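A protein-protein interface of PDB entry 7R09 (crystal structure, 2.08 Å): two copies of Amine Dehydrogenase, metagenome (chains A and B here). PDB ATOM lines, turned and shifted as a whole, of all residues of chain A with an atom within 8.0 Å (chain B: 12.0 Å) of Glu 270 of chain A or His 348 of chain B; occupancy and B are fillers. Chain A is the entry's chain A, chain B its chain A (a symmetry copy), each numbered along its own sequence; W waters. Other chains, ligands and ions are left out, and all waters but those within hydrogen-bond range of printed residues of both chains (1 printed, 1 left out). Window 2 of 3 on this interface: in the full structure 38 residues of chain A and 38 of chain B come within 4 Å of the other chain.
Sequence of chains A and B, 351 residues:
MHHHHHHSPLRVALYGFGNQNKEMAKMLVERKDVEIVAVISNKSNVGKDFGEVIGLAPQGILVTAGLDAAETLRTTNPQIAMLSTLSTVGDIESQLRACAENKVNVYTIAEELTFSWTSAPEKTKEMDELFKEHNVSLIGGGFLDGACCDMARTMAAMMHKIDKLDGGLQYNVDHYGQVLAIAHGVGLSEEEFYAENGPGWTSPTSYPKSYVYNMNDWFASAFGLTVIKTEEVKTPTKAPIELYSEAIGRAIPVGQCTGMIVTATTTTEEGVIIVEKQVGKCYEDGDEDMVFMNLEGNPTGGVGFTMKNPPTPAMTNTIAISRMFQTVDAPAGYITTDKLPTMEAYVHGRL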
ATOM      1  N   HIS A 160     -24.453  36.128  24.762  1.00  0.00           N
ATOM      2  CA  HIS A 160     -25.488  35.891  25.811  1.00  0.00           C
ATOM      3  C   HIS A 160     -26.673  35.162  25.167  1.00  0.00           C
ATOM      4  O   HIS A 160     -27.102  34.138  25.713  1.00  0.00           O
ATOM      5  CB  HIS A 160     -25.846  37.224  26.474  1.00  0.00           C
ATOM      6  CG  HIS A 160     -27.003  37.184  27.408  1.00  0.00           C
ATOM      7  ND1 HIS A 160     -26.954  36.522  28.611  1.00  0.00           N
ATOM      8  CD2 HIS A 160     -28.219  37.767  27.333  1.00  0.00           C
ATOM      9  CE1 HIS A 160     -28.095  36.697  29.242  1.00  0.00           C
ATOM     10  NE2 HIS A 160     -28.887  37.440  28.473  1.00  0.00           N
ATOM     11  N   LYS A 161     -27.144  35.654  24.018  1.00  0.00           N
ATOM     12  CA  LYS A 161     -28.166  34.965  23.192  1.00  0.00           C
ATOM     13  C   LYS A 161     -27.707  34.972  21.735  1.00  0.00           C
ATOM     14  O   LYS A 161     -27.381  36.048  21.235  1.00  0.00           O
ATOM     15  CB  LYS A 161     -29.536  35.650  23.311  1.00  0.00           C
ATOM     16  N   ILE A 162     -27.784  33.833  21.050  1.00  0.00           N
ATOM     17  CA  ILE A 162     -27.599  33.803  19.572  1.00  0.00           C
ATOM     18  C   ILE A 162     -28.955  33.520  18.911  1.00  0.00           C
ATOM     19  O   ILE A 162     -29.573  32.446  19.205  1.00  0.00           O
ATOM     20  CB  ILE A 162     -26.484  32.820  19.158  1.00  0.00           C
ATOM     21  CG1 ILE A 162     -26.565  32.459  17.679  1.00  0.00           C
ATOM     22  CG2 ILE A 162     -26.468  31.588  20.020  1.00  0.00           C
ATOM     23  CD1 ILE A 162     -26.083  33.570  16.817  1.00  0.00           C
ATOM     24  N   ASP A 163     -29.373  34.458  18.049  1.00  0.00           N
ATOM     25  CA  ASP A 163     -30.562  34.392  17.161  1.00  0.00           C
ATOM     26  C   ASP A 163     -30.194  33.769  15.806  1.00  0.00           C
ATOM     27  O   ASP A 163     -31.044  33.044  15.229  1.00  0.00           O
ATOM     28  CB  ASP A 163     -31.139  35.789  16.954  1.00  0.00           C
ATOM     29  CG  ASP A 163     -31.611  36.438  18.248  1.00  0.00           C
ATOM     30  OD1 ASP A 163     -32.023  35.698  19.149  1.00  0.00           O
ATOM     31  OD2 ASP A 163     -31.551  37.673  18.347  1.00  0.00           O
ATOM     32  N   ALA A 220     -25.328  23.202  15.276  1.00  0.00           N
ATOM     33  CA  ALA A 220     -26.596  22.782  15.918  1.00  0.00           C
ATOM     34  C   ALA A 220     -26.259  21.880  17.103  1.00  0.00           C
ATOM     35  O   ALA A 220     -26.799  22.113  18.190  1.00  0.00           O
ATOM     36  CB  ALA A 220     -27.493  22.097  14.925  1.00  0.00           C
ATOM     37  N   SER A 221     -25.368  20.906  16.907  1.00  0.00           N
ATOM     38  CA  SER A 221     -24.837  20.082  18.024  1.00  0.00           C
ATOM     39  C   SER A 221     -24.154  20.996  19.050  1.00  0.00           C
ATOM     40  O   SER A 221     -24.548  20.964  20.223  1.00  0.00           O
ATOM     41  CB  SER A 221     -23.929  19.005  17.528  1.00  0.00           C
ATOM     42  OG  SER A 221     -23.466  18.211  18.613  1.00  0.00           O
ATOM     43  N   ALA A 222     -23.190  21.816  18.622  1.00  0.00           N
ATOM     44  CA  ALA A 222     -22.400  22.694  19.519  1.00  0.00           C
ATOM     45  C   ALA A 222     -23.340  23.524  20.402  1.00  0.00           C
ATOM     46  O   ALA A 222     -23.151  23.551  21.599  1.00  0.00           O
ATOM     47  CB  ALA A 222     -21.509  23.605  18.710  1.00  0.00           C
ATOM     48  N   PHE A 223     -24.315  24.201  19.810  1.00  0.00           N
ATOM     49  CA  PHE A 223     -25.184  25.160  20.531  1.00  0.00           C
ATOM     50  C   PHE A 223     -26.329  24.424  21.247  1.00  0.00           C
ATOM     51  O   PHE A 223     -27.129  25.120  21.843  1.00  0.00           O
ATOM     52  CB  PHE A 223     -25.659  26.259  19.571  1.00  0.00           C
ATOM     53  CG  PHE A 223     -24.562  27.075  18.924  1.00  0.00           C
ATOM     54  CD1 PHE A 223     -23.280  27.140  19.474  1.00  0.00           C
ATOM     55  CD2 PHE A 223     -24.810  27.786  17.758  1.00  0.00           C
ATOM     56  CE1 PHE A 223     -22.290  27.922  18.891  1.00  0.00           C
ATOM     57  CE2 PHE A 223     -23.814  28.558  17.169  1.00  0.00           C
ATOM     58  CZ  PHE A 223     -22.558  28.628  17.737  1.00  0.00           C
ATOM     59  N   GLY A 224     -26.372  23.086  21.249  1.00  0.00           N
ATOM     60  CA  GLY A 224     -27.474  22.299  21.849  1.00  0.00           C
ATOM     61  C   GLY A 224     -28.843  22.648  21.261  1.00  0.00           C
ATOM     62  O   GLY A 224     -29.791  22.848  22.038  1.00  0.00           O
ATOM     63  N   LEU A 225     -28.960  22.745  19.934  1.00  0.00           N
ATOM     64  CA  LEU A 225     -30.243  23.054  19.247  1.00  0.00           C
ATOM     65  C   LEU A 225     -30.819  21.774  18.617  1.00  0.00           C
ATOM     66  O   LEU A 225     -30.085  20.786  18.438  1.00  0.00           O
ATOM     67  CB  LEU A 225     -30.023  24.125  18.172  1.00  0.00           C
ATOM     68  CG  LEU A 225     -29.432  25.458  18.640  1.00  0.00           C
ATOM     69  CD1 LEU A 225     -28.874  26.251  17.448  1.00  0.00           C
ATOM     70  CD2 LEU A 225     -30.474  26.271  19.392  1.00  0.00           C
ATOM     71  N   THR A 226     -32.088  21.832  18.225  1.00  0.00           N
ATOM     72  CA  THR A 226     -32.842  20.707  17.623  1.00  0.00           C
ATOM     73  C   THR A 226     -33.131  21.071  16.173  1.00  0.00           C
ATOM     74  O   THR A 226     -33.936  22.009  15.960  1.00  0.00           O
ATOM     75  CB  THR A 226     -34.114  20.434  18.432  1.00  0.00           C
ATOM     76  OG1 THR A 226     -33.746  20.440  19.815  1.00  0.00           O
ATOM     77  CG2 THR A 226     -34.761  19.116  18.066  1.00  0.00           C
ATOM     78  N   VAL A 227     -32.489  20.380  15.226  1.00  0.00           N
ATOM     79  CA  VAL A 227     -32.643  20.682  13.770  1.00  0.00           C
ATOM     80  C   VAL A 227     -34.059  20.296  13.341  1.00  0.00           C
ATOM     81  O   VAL A 227     -34.450  19.158  13.626  1.00  0.00           O
ATOM     82  CB  VAL A 227     -31.616  19.953  12.893  1.00  0.00           C
ATOM     83  CG1 VAL A 227     -31.861  20.250  11.417  1.00  0.00           C
ATOM     84  CG2 VAL A 227     -30.186  20.309  13.274  1.00  0.00           C
ATOM     85  N   ILE A 228     -34.761  21.210  12.668  1.00  0.00           N
ATOM     86  CA  ILE A 228     -35.999  20.905  11.896  1.00  0.00           C
ATOM     87  C   ILE A 228     -35.569  20.401  10.518  1.00  0.00           C
ATOM     88  O   ILE A 228     -35.912  19.280  10.159  1.00  0.00           O
ATOM     89  CB  ILE A 228     -36.912  22.140  11.790  1.00  0.00           C
ATOM     90  CG1 ILE A 228     -37.523  22.511  13.144  1.00  0.00           C
ATOM     91  CG2 ILE A 228     -37.981  21.936  10.720  1.00  0.00           C
ATOM     92  CD1 ILE A 228     -38.503  23.678  13.073  1.00  0.00           C
ATOM     93  N   THR A 267     -33.002  25.444   9.955  1.00  0.00           N
ATOM     94  CA  THR A 267     -33.966  25.896  10.995  1.00  0.00           C
ATOM     95  C   THR A 267     -33.922  24.904  12.153  1.00  0.00           C
ATOM     96  O   THR A 267     -33.666  23.716  11.900  1.00  0.00           O
ATOM     97  CB  THR A 267     -35.381  26.018  10.438  1.00  0.00           C
ATOM     98  OG1 THR A 267     -35.582  24.808   9.709  1.00  0.00           O
ATOM     99  CG2 THR A 267     -35.558  27.248   9.575  1.00  0.00           C
ATOM    100  N   THR A 268     -34.179  25.388  13.366  1.00  0.00           N
ATOM    101  CA  THR A 268     -34.172  24.593  14.618  1.00  0.00           C
ATOM    102  C   THR A 268     -35.502  24.815  15.348  1.00  0.00           C
ATOM    103  O   THR A 268     -36.147  25.834  15.055  1.00  0.00           O
ATOM    104  CB  THR A 268     -32.980  25.022  15.483  1.00  0.00           C
ATOM    105  OG1 THR A 268     -33.164  26.386  15.859  1.00  0.00           O
ATOM    106  CG2 THR A 268     -31.658  24.911  14.757  1.00  0.00           C
ATOM    107  N   GLU A 269     -35.845  23.957  16.312  1.00  0.00           N
ATOM    108  CA  GLU A 269     -37.071  24.108  17.144  1.00  0.00           C
ATOM    109  C   GLU A 269     -36.957  25.347  18.044  1.00  0.00           C
ATOM    110  O   GLU A 269     -38.004  25.970  18.344  1.00  0.00           O
ATOM    111  CB  GLU A 269     -37.304  22.861  17.992  1.00  0.00           C
ATOM    112  CG  GLU A 269     -37.756  21.654  17.188  1.00  0.00           C
ATOM    113  CD  GLU A 269     -37.807  20.374  18.008  1.00  0.00           C
ATOM    114  OE1 GLU A 269     -37.750  20.472  19.255  1.00  0.00           O
ATOM    115  OE2 GLU A 269     -37.883  19.277  17.404  1.00  0.00           O
ATOM    116  N   GLU A 270     -35.738  25.731  18.443  1.00  0.00           N
ATOM    117  CA  GLU A 270     -35.539  26.849  19.407  1.00  0.00           C
ATOM    118  C   GLU A 270     -35.585  28.189  18.675  1.00  0.00           C
ATOM    119  O   GLU A 270     -35.498  29.215  19.360  1.00  0.00           O
ATOM    120  CB  GLU A 270     -34.261  26.628  20.199  1.00  0.00           C
ATOM    121  CG  GLU A 270     -34.248  25.281  20.914  1.00  0.00           C
ATOM    122  CD  GLU A 270     -33.830  24.099  20.065  1.00  0.00           C
ATOM    123  OE1 GLU A 270     -33.697  24.281  18.848  1.00  0.00           O
ATOM    124  OE2 GLU A 270     -33.615  23.005  20.624  1.00  0.00           O
ATOM    125  N   GLY A 271     -35.813  28.196  17.356  1.00  0.00           N
ATOM    126  CA  GLY A 271     -35.990  29.440  16.579  1.00  0.00           C
ATOM    127  C   GLY A 271     -34.671  30.032  16.088  1.00  0.00           C
ATOM    128  O   GLY A 271     -34.720  31.084  15.412  1.00  0.00           O
ATOM    129  N   VAL A 272     -33.540  29.376  16.367  1.00  0.00           N
ATOM    130  CA  VAL A 272     -32.177  29.831  15.947  1.00  0.00           C
ATOM    131  C   VAL A 272     -31.936  29.405  14.505  1.00  0.00           C
ATOM    132  O   VAL A 272     -32.158  28.229  14.200  1.00  0.00           O
ATOM    133  CB  VAL A 272     -31.094  29.285  16.889  1.00  0.00           C
ATOM    134  CG1 VAL A 272     -29.692  29.691  16.459  1.00  0.00           C
ATOM    135  CG2 VAL A 272     -31.370  29.740  18.310  1.00  0.00           C
ATOM    136  N   ILE A 273     -31.574  30.359  13.647  1.00  0.00           N
ATOM    137  CA  ILE A 273     -31.275  30.123  12.208  1.00  0.00           C
ATOM    138  C   ILE A 273     -29.748  29.993  12.025  1.00  0.00           C
ATOM    139  O   ILE A 273     -29.002  30.807  12.631  1.00  0.00           O
ATOM    140  CB  ILE A 273     -31.891  31.277  11.391  1.00  0.00           C
ATOM    141  CG1 ILE A 273     -33.414  31.322  11.587  1.00  0.00           C
ATOM    142  CG2 ILE A 273     -31.526  31.173   9.922  1.00  0.00           C
ATOM    143  CD1 ILE A 273     -34.065  32.538  10.982  1.00  0.00           C
ATOM    144  N   GLU B  30     -31.131  37.053  33.965  1.00  0.00           N
ATOM    145  CA  GLU B  30     -31.784  36.204  32.926  1.00  0.00           C
ATOM    146  C   GLU B  30     -31.230  34.787  32.964  1.00  0.00           C
ATOM    147  O   GLU B  30     -31.862  33.903  32.399  1.00  0.00           O
ATOM    148  CB  GLU B  30     -31.553  36.775  31.532  1.00  0.00           C
ATOM    149  CG  GLU B  30     -32.404  37.999  31.252  1.00  0.00           C
ATOM    150  CD  GLU B  30     -32.288  38.510  29.830  1.00  0.00           C
ATOM    151  OE1 GLU B  30     -31.470  37.949  29.089  1.00  0.00           O
ATOM    152  OE2 GLU B  30     -33.004  39.466  29.472  1.00  0.00           O
ATOM    153  N   ARG B  31     -30.085  34.591  33.598  1.00  0.00           N
ATOM    154  CA  ARG B  31     -29.375  33.296  33.607  1.00  0.00           C
ATOM    155  C   ARG B  31     -29.837  32.476  34.820  1.00  0.00           C
ATOM    156  O   ARG B  31     -29.515  32.881  35.957  1.00  0.00           O
ATOM    157  CB  ARG B  31     -27.874  33.576  33.599  1.00  0.00           C
ATOM    158  CG  ARG B  31     -27.033  32.319  33.535  1.00  0.00           C
ATOM    159  CD  ARG B  31     -26.622  32.028  32.117  1.00  0.00           C
ATOM    160  NE  ARG B  31     -25.426  31.221  32.192  1.00  0.00           N
ATOM    161  CZ  ARG B  31     -24.303  31.476  31.557  1.00  0.00           C
ATOM    162  NH1 ARG B  31     -24.221  32.514  30.746  1.00  0.00           N
ATOM    163  NH2 ARG B  31     -23.268  30.668  31.711  1.00  0.00           N
ATOM    164  N   LYS B  32     -30.565  31.375  34.576  1.00  0.00           N
ATOM    165  CA  LYS B  32     -31.188  30.496  35.607  1.00  0.00           C
ATOM    166  C   LYS B  32     -30.088  29.691  36.303  1.00  0.00           C
ATOM    167  O   LYS B  32     -30.362  29.022  37.326  1.00  0.00           O
ATOM    168  CB  LYS B  32     -32.212  29.552  34.963  1.00  0.00           C
ATOM    169  N   ASP B  33     -28.898  29.757  35.720  1.00  0.00           N
ATOM    170  CA  ASP B  33     -27.644  29.109  36.161  1.00  0.00           C
ATOM    171  C   ASP B  33     -27.073  29.854  37.381  1.00  0.00           C
ATOM    172  O   ASP B  33     -26.208  29.280  38.071  1.00  0.00           O
ATOM    173  CB  ASP B  33     -26.669  29.163  34.979  1.00  0.00           C
ATOM    174  CG  ASP B  33     -25.556  28.142  35.023  1.00  0.00           C
ATOM    175  OD1 ASP B  33     -25.621  27.238  35.885  1.00  0.00           O
ATOM    176  OD2 ASP B  33     -24.640  28.258  34.176  1.00  0.00           O
ATOM    177  N   GLU B 344     -15.993  29.494  28.338  1.00  0.00           N
ATOM    178  CA  GLU B 344     -17.041  28.431  28.367  1.00  0.00           C
ATOM    179  C   GLU B 344     -17.974  28.600  27.160  1.00  0.00           C
ATOM    180  O   GLU B 344     -18.417  29.732  26.914  1.00  0.00           O
ATOM    181  CB  GLU B 344     -17.812  28.473  29.688  1.00  0.00           C
ATOM    182  CG  GLU B 344     -18.807  27.338  29.870  1.00  0.00           C
ATOM    183  CD  GLU B 344     -18.183  25.959  29.896  1.00  0.00           C
ATOM    184  OE1 GLU B 344     -17.093  25.816  30.500  1.00  0.00           O
ATOM    185  OE2 GLU B 344     -18.771  25.039  29.279  1.00  0.00           O
ATOM    186  N   ALA B 345     -18.262  27.502  26.445  1.00  0.00           N
ATOM    187  CA  ALA B 345     -18.895  27.515  25.111  1.00  0.00           C
ATOM    188  C   ALA B 345     -20.331  28.000  25.256  1.00  0.00           C
ATOM    189  O   ALA B 345     -20.955  27.754  26.305  1.00  0.00           O
ATOM    190  CB  ALA B 345     -18.861  26.148  24.476  1.00  0.00           C
ATOM    191  N   TYR B 346     -20.831  28.665  24.229  1.00  0.00           N
ATOM    192  CA  TYR B 346     -22.257  29.019  24.110  1.00  0.00           C
ATOM    193  C   TYR B 346     -23.106  27.751  23.936  1.00  0.00           C
ATOM    194  O   TYR B 346     -22.855  26.958  23.010  1.00  0.00           O
ATOM    195  CB  TYR B 346     -22.501  29.917  22.904  1.00  0.00           C
ATOM    196  CG  TYR B 346     -23.944  30.290  22.811  1.00  0.00           C
ATOM    197  CD1 TYR B 346     -24.422  31.403  23.483  1.00  0.00           C
ATOM    198  CD2 TYR B 346     -24.850  29.467  22.161  1.00  0.00           C
ATOM    199  CE1 TYR B 346     -25.764  31.740  23.451  1.00  0.00           C
ATOM    200  CE2 TYR B 346     -26.191  29.799  22.103  1.00  0.00           C
ATOM    201  CZ  TYR B 346     -26.647  30.930  22.759  1.00  0.00           C
ATOM    202  OH  TYR B 346     -27.958  31.271  22.709  1.00  0.00           O
ATOM    203  N   VAL B 347     -24.140  27.621  24.768  1.00  0.00           N
ATOM    204  CA  VAL B 347     -25.196  26.577  24.654  1.00  0.00           C
ATOM    205  C   VAL B 347     -26.547  27.257  24.880  1.00  0.00           C
ATOM    206  O   VAL B 347     -26.634  28.049  25.812  1.00  0.00           O
ATOM    207  CB  VAL B 347     -24.946  25.440  25.661  1.00  0.00           C
ATOM    208  CG1 VAL B 347     -23.641  24.711  25.370  1.00  0.00           C
ATOM    209  CG2 VAL B 347     -24.952  25.945  27.091  1.00  0.00           C
ATOM    210  N   HIS B 348     -27.550  26.960  24.050  1.00  0.00           N
ATOM    211  CA  HIS B 348     -28.973  27.337  24.273  1.00  0.00           C
ATOM    212  C   HIS B 348     -29.501  26.736  25.588  1.00  0.00           C
ATOM    213  O   HIS B 348     -29.025  25.675  25.992  1.00  0.00           O
ATOM    214  CB  HIS B 348     -29.820  26.900  23.073  1.00  0.00           C
ATOM    215  CG  HIS B 348     -31.247  27.326  23.174  1.00  0.00           C
ATOM    216  ND1 HIS B 348     -32.210  26.557  23.830  1.00  0.00           N
ATOM    217  CD2 HIS B 348     -31.876  28.419  22.701  1.00  0.00           C
ATOM    218  CE1 HIS B 348     -33.369  27.163  23.752  1.00  0.00           C
ATOM    219  NE2 HIS B 348     -33.196  28.302  23.047  1.00  0.00           N
ATOM    220  N   GLY B 349     -30.457  27.403  26.245  1.00  0.00           N
ATOM    221  CA  GLY B 349     -31.228  26.853  27.380  1.00  0.00           C
ATOM    222  C   GLY B 349     -30.737  27.327  28.739  1.00  0.00           C
ATOM    223  O   GLY B 349     -31.167  26.744  29.752  1.00  0.00           O
ATOM    224  N   ARG B 350     -29.858  28.333  28.774  1.00  0.00           N
ATOM    225  CA  ARG B 350     -29.446  29.032  30.019  1.00  0.00           C
ATOM    226  C   ARG B 350     -30.320  30.281  30.210  1.00  0.00           C
ATOM    227  O   ARG B 350     -30.379  30.774  31.346  1.00  0.00           O
ATOM    228  CB  ARG B 350     -27.967  29.433  29.958  1.00  0.00           C
ATOM    229  CG  ARG B 350     -27.022  28.372  29.408  1.00  0.00           C
ATOM    230  CD  ARG B 350     -25.581  28.514  29.897  1.00  0.00           C
ATOM    231  NE  ARG B 350     -24.544  28.812  28.904  1.00  0.00           N
ATOM    232  CZ  ARG B 350     -24.469  29.911  28.171  1.00  0.00           C
ATOM    233  NH1 ARG B 350     -25.409  30.838  28.247  1.00  0.00           N
ATOM    234  NH2 ARG B 350     -23.468  30.071  27.330  1.00  0.00           N
ATOM    235  N   LEU B 351     -30.963  30.747  29.133  1.00  0.00           N
ATOM    236  CA  LEU B 351     -31.795  31.974  29.025  1.00  0.00           C
ATOM    237  C   LEU B 351     -30.891  33.211  29.018  1.00  0.00           C
ATOM    238  O   LEU B 351     -30.679  33.783  27.942  1.00  0.00           O
ATOM    239  CB  LEU B 351     -32.816  32.009  30.166  1.00  0.00           C
ATOM    240  CG  LEU B 351     -33.860  30.892  30.173  1.00  0.00           C
ATOM    241  CD1 LEU B 351     -34.206  30.438  28.768  1.00  0.00           C
ATOM    242  CD2 LEU B 351     -33.407  29.698  31.001  1.00  0.00           C
HETATM  243  O   HOH W   1     -28.876  32.125  25.240  1.00  0.00           O
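No position is printed for both chains. Of the 11 pairs that touch across the chains among the printed residues, none has its exchanged pair printed and touching as well.
Among the printed residues, merely in contact across the chains: Glu 270 of chain A with His 348 of chain B, His 160 of chain A with Tyr 346 of chain B, Phe 223 of chain A with Tyr 346 of chain B, Ala 222 of chain A with Tyr 346 of chain B, Phe 223 of chain A with Val 347 of chain B, Lys 161 of chain A with Tyr 346 of chain B, Leu 225 of chain A with His 348 of chain B and Ala 222 of chain A with Val 347 of chain B.
Of the 12 printed residues of chain B, 4 touch a printed residue of chain A. Hydrophobic or aromatic side chains of chain B that line the printed part of chain A: Tyr 346, Val 347 and His 348. Among the printed residues, 11 pairs touch across the chains. Among the printed residues, no Asp or Glu carboxylate lies within 4 Å of a Lys or Arg side-chain nitrogen of the other chain.
Water W1 bridges O of His 160 of chain A (2.7 Å) and OH of Tyr 346 of chain B (2.8 Å).
Glu 270 of chain A touches just one residue of chain B: His 348 (3.5 Å). Of chain A, only Phe 223, Leu 225 and Glu 270 come within 4 Å of His 348 of chain B. No residue of chain B comes within 4 Å of Thr 226 of chain A. Gly 271 of chain A touches none of the printed residues of chain B. Val 272 of chain A touches none of the printed residues of chain B. Printed residues of chain A within 4 Å of Val 347 of chain B: Ala 222 (3.98 Å) and Phe 223 (3.7 Å). Of the printed residues of chain B, His 160 of chain A touches Glu 30 (2.7 Å) and Tyr 346 (3.6 Å). Of the printed residues of chain B, Phe 223 of chain A touches Tyr 346 (3.6 Å), Val 347 (3.7 Å) and His 348 (2.9 Å). Of the printed residues of chain B, Ile 162 of chain A touches Tyr 346. Glu 344 of chain B touches none of the printed residues of chain A. Ser 221 of chain A touches none of the printed residues of chain B. The nearest residue of chain B that does not touch Glu 270 of chain A is Gly 349 of chain B (6.9 Å). The nearest residue of chain A that does not touch His 348 of chain B is Gly 224 of chain A (4.2 Å).
O of Ala 220 of chain A sits at hydrogen-bond distance from N of Leu 225 of chain A (2.8 Å). The side-chain hydroxyl (OG1) of Thr 226 of chain A sits at hydrogen-bond distance from the side-chain carboxylate (OE2) of Glu 270 of chain A, at 2.7 Å.
OE1 of Glu 30 of chain B lies within hydrogen-bond range of NE2 of His 160 of chain A (2.7 Å). The side-chain hydroxyl (OH) of Tyr 346 of chain B lies within hydrogen-bond range of the backbone NH (N) of Ile 162 of chain A (3.1 Å). O of Phe 223 of chain A lies within hydrogen-bond range of N of His 348 of chain B.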
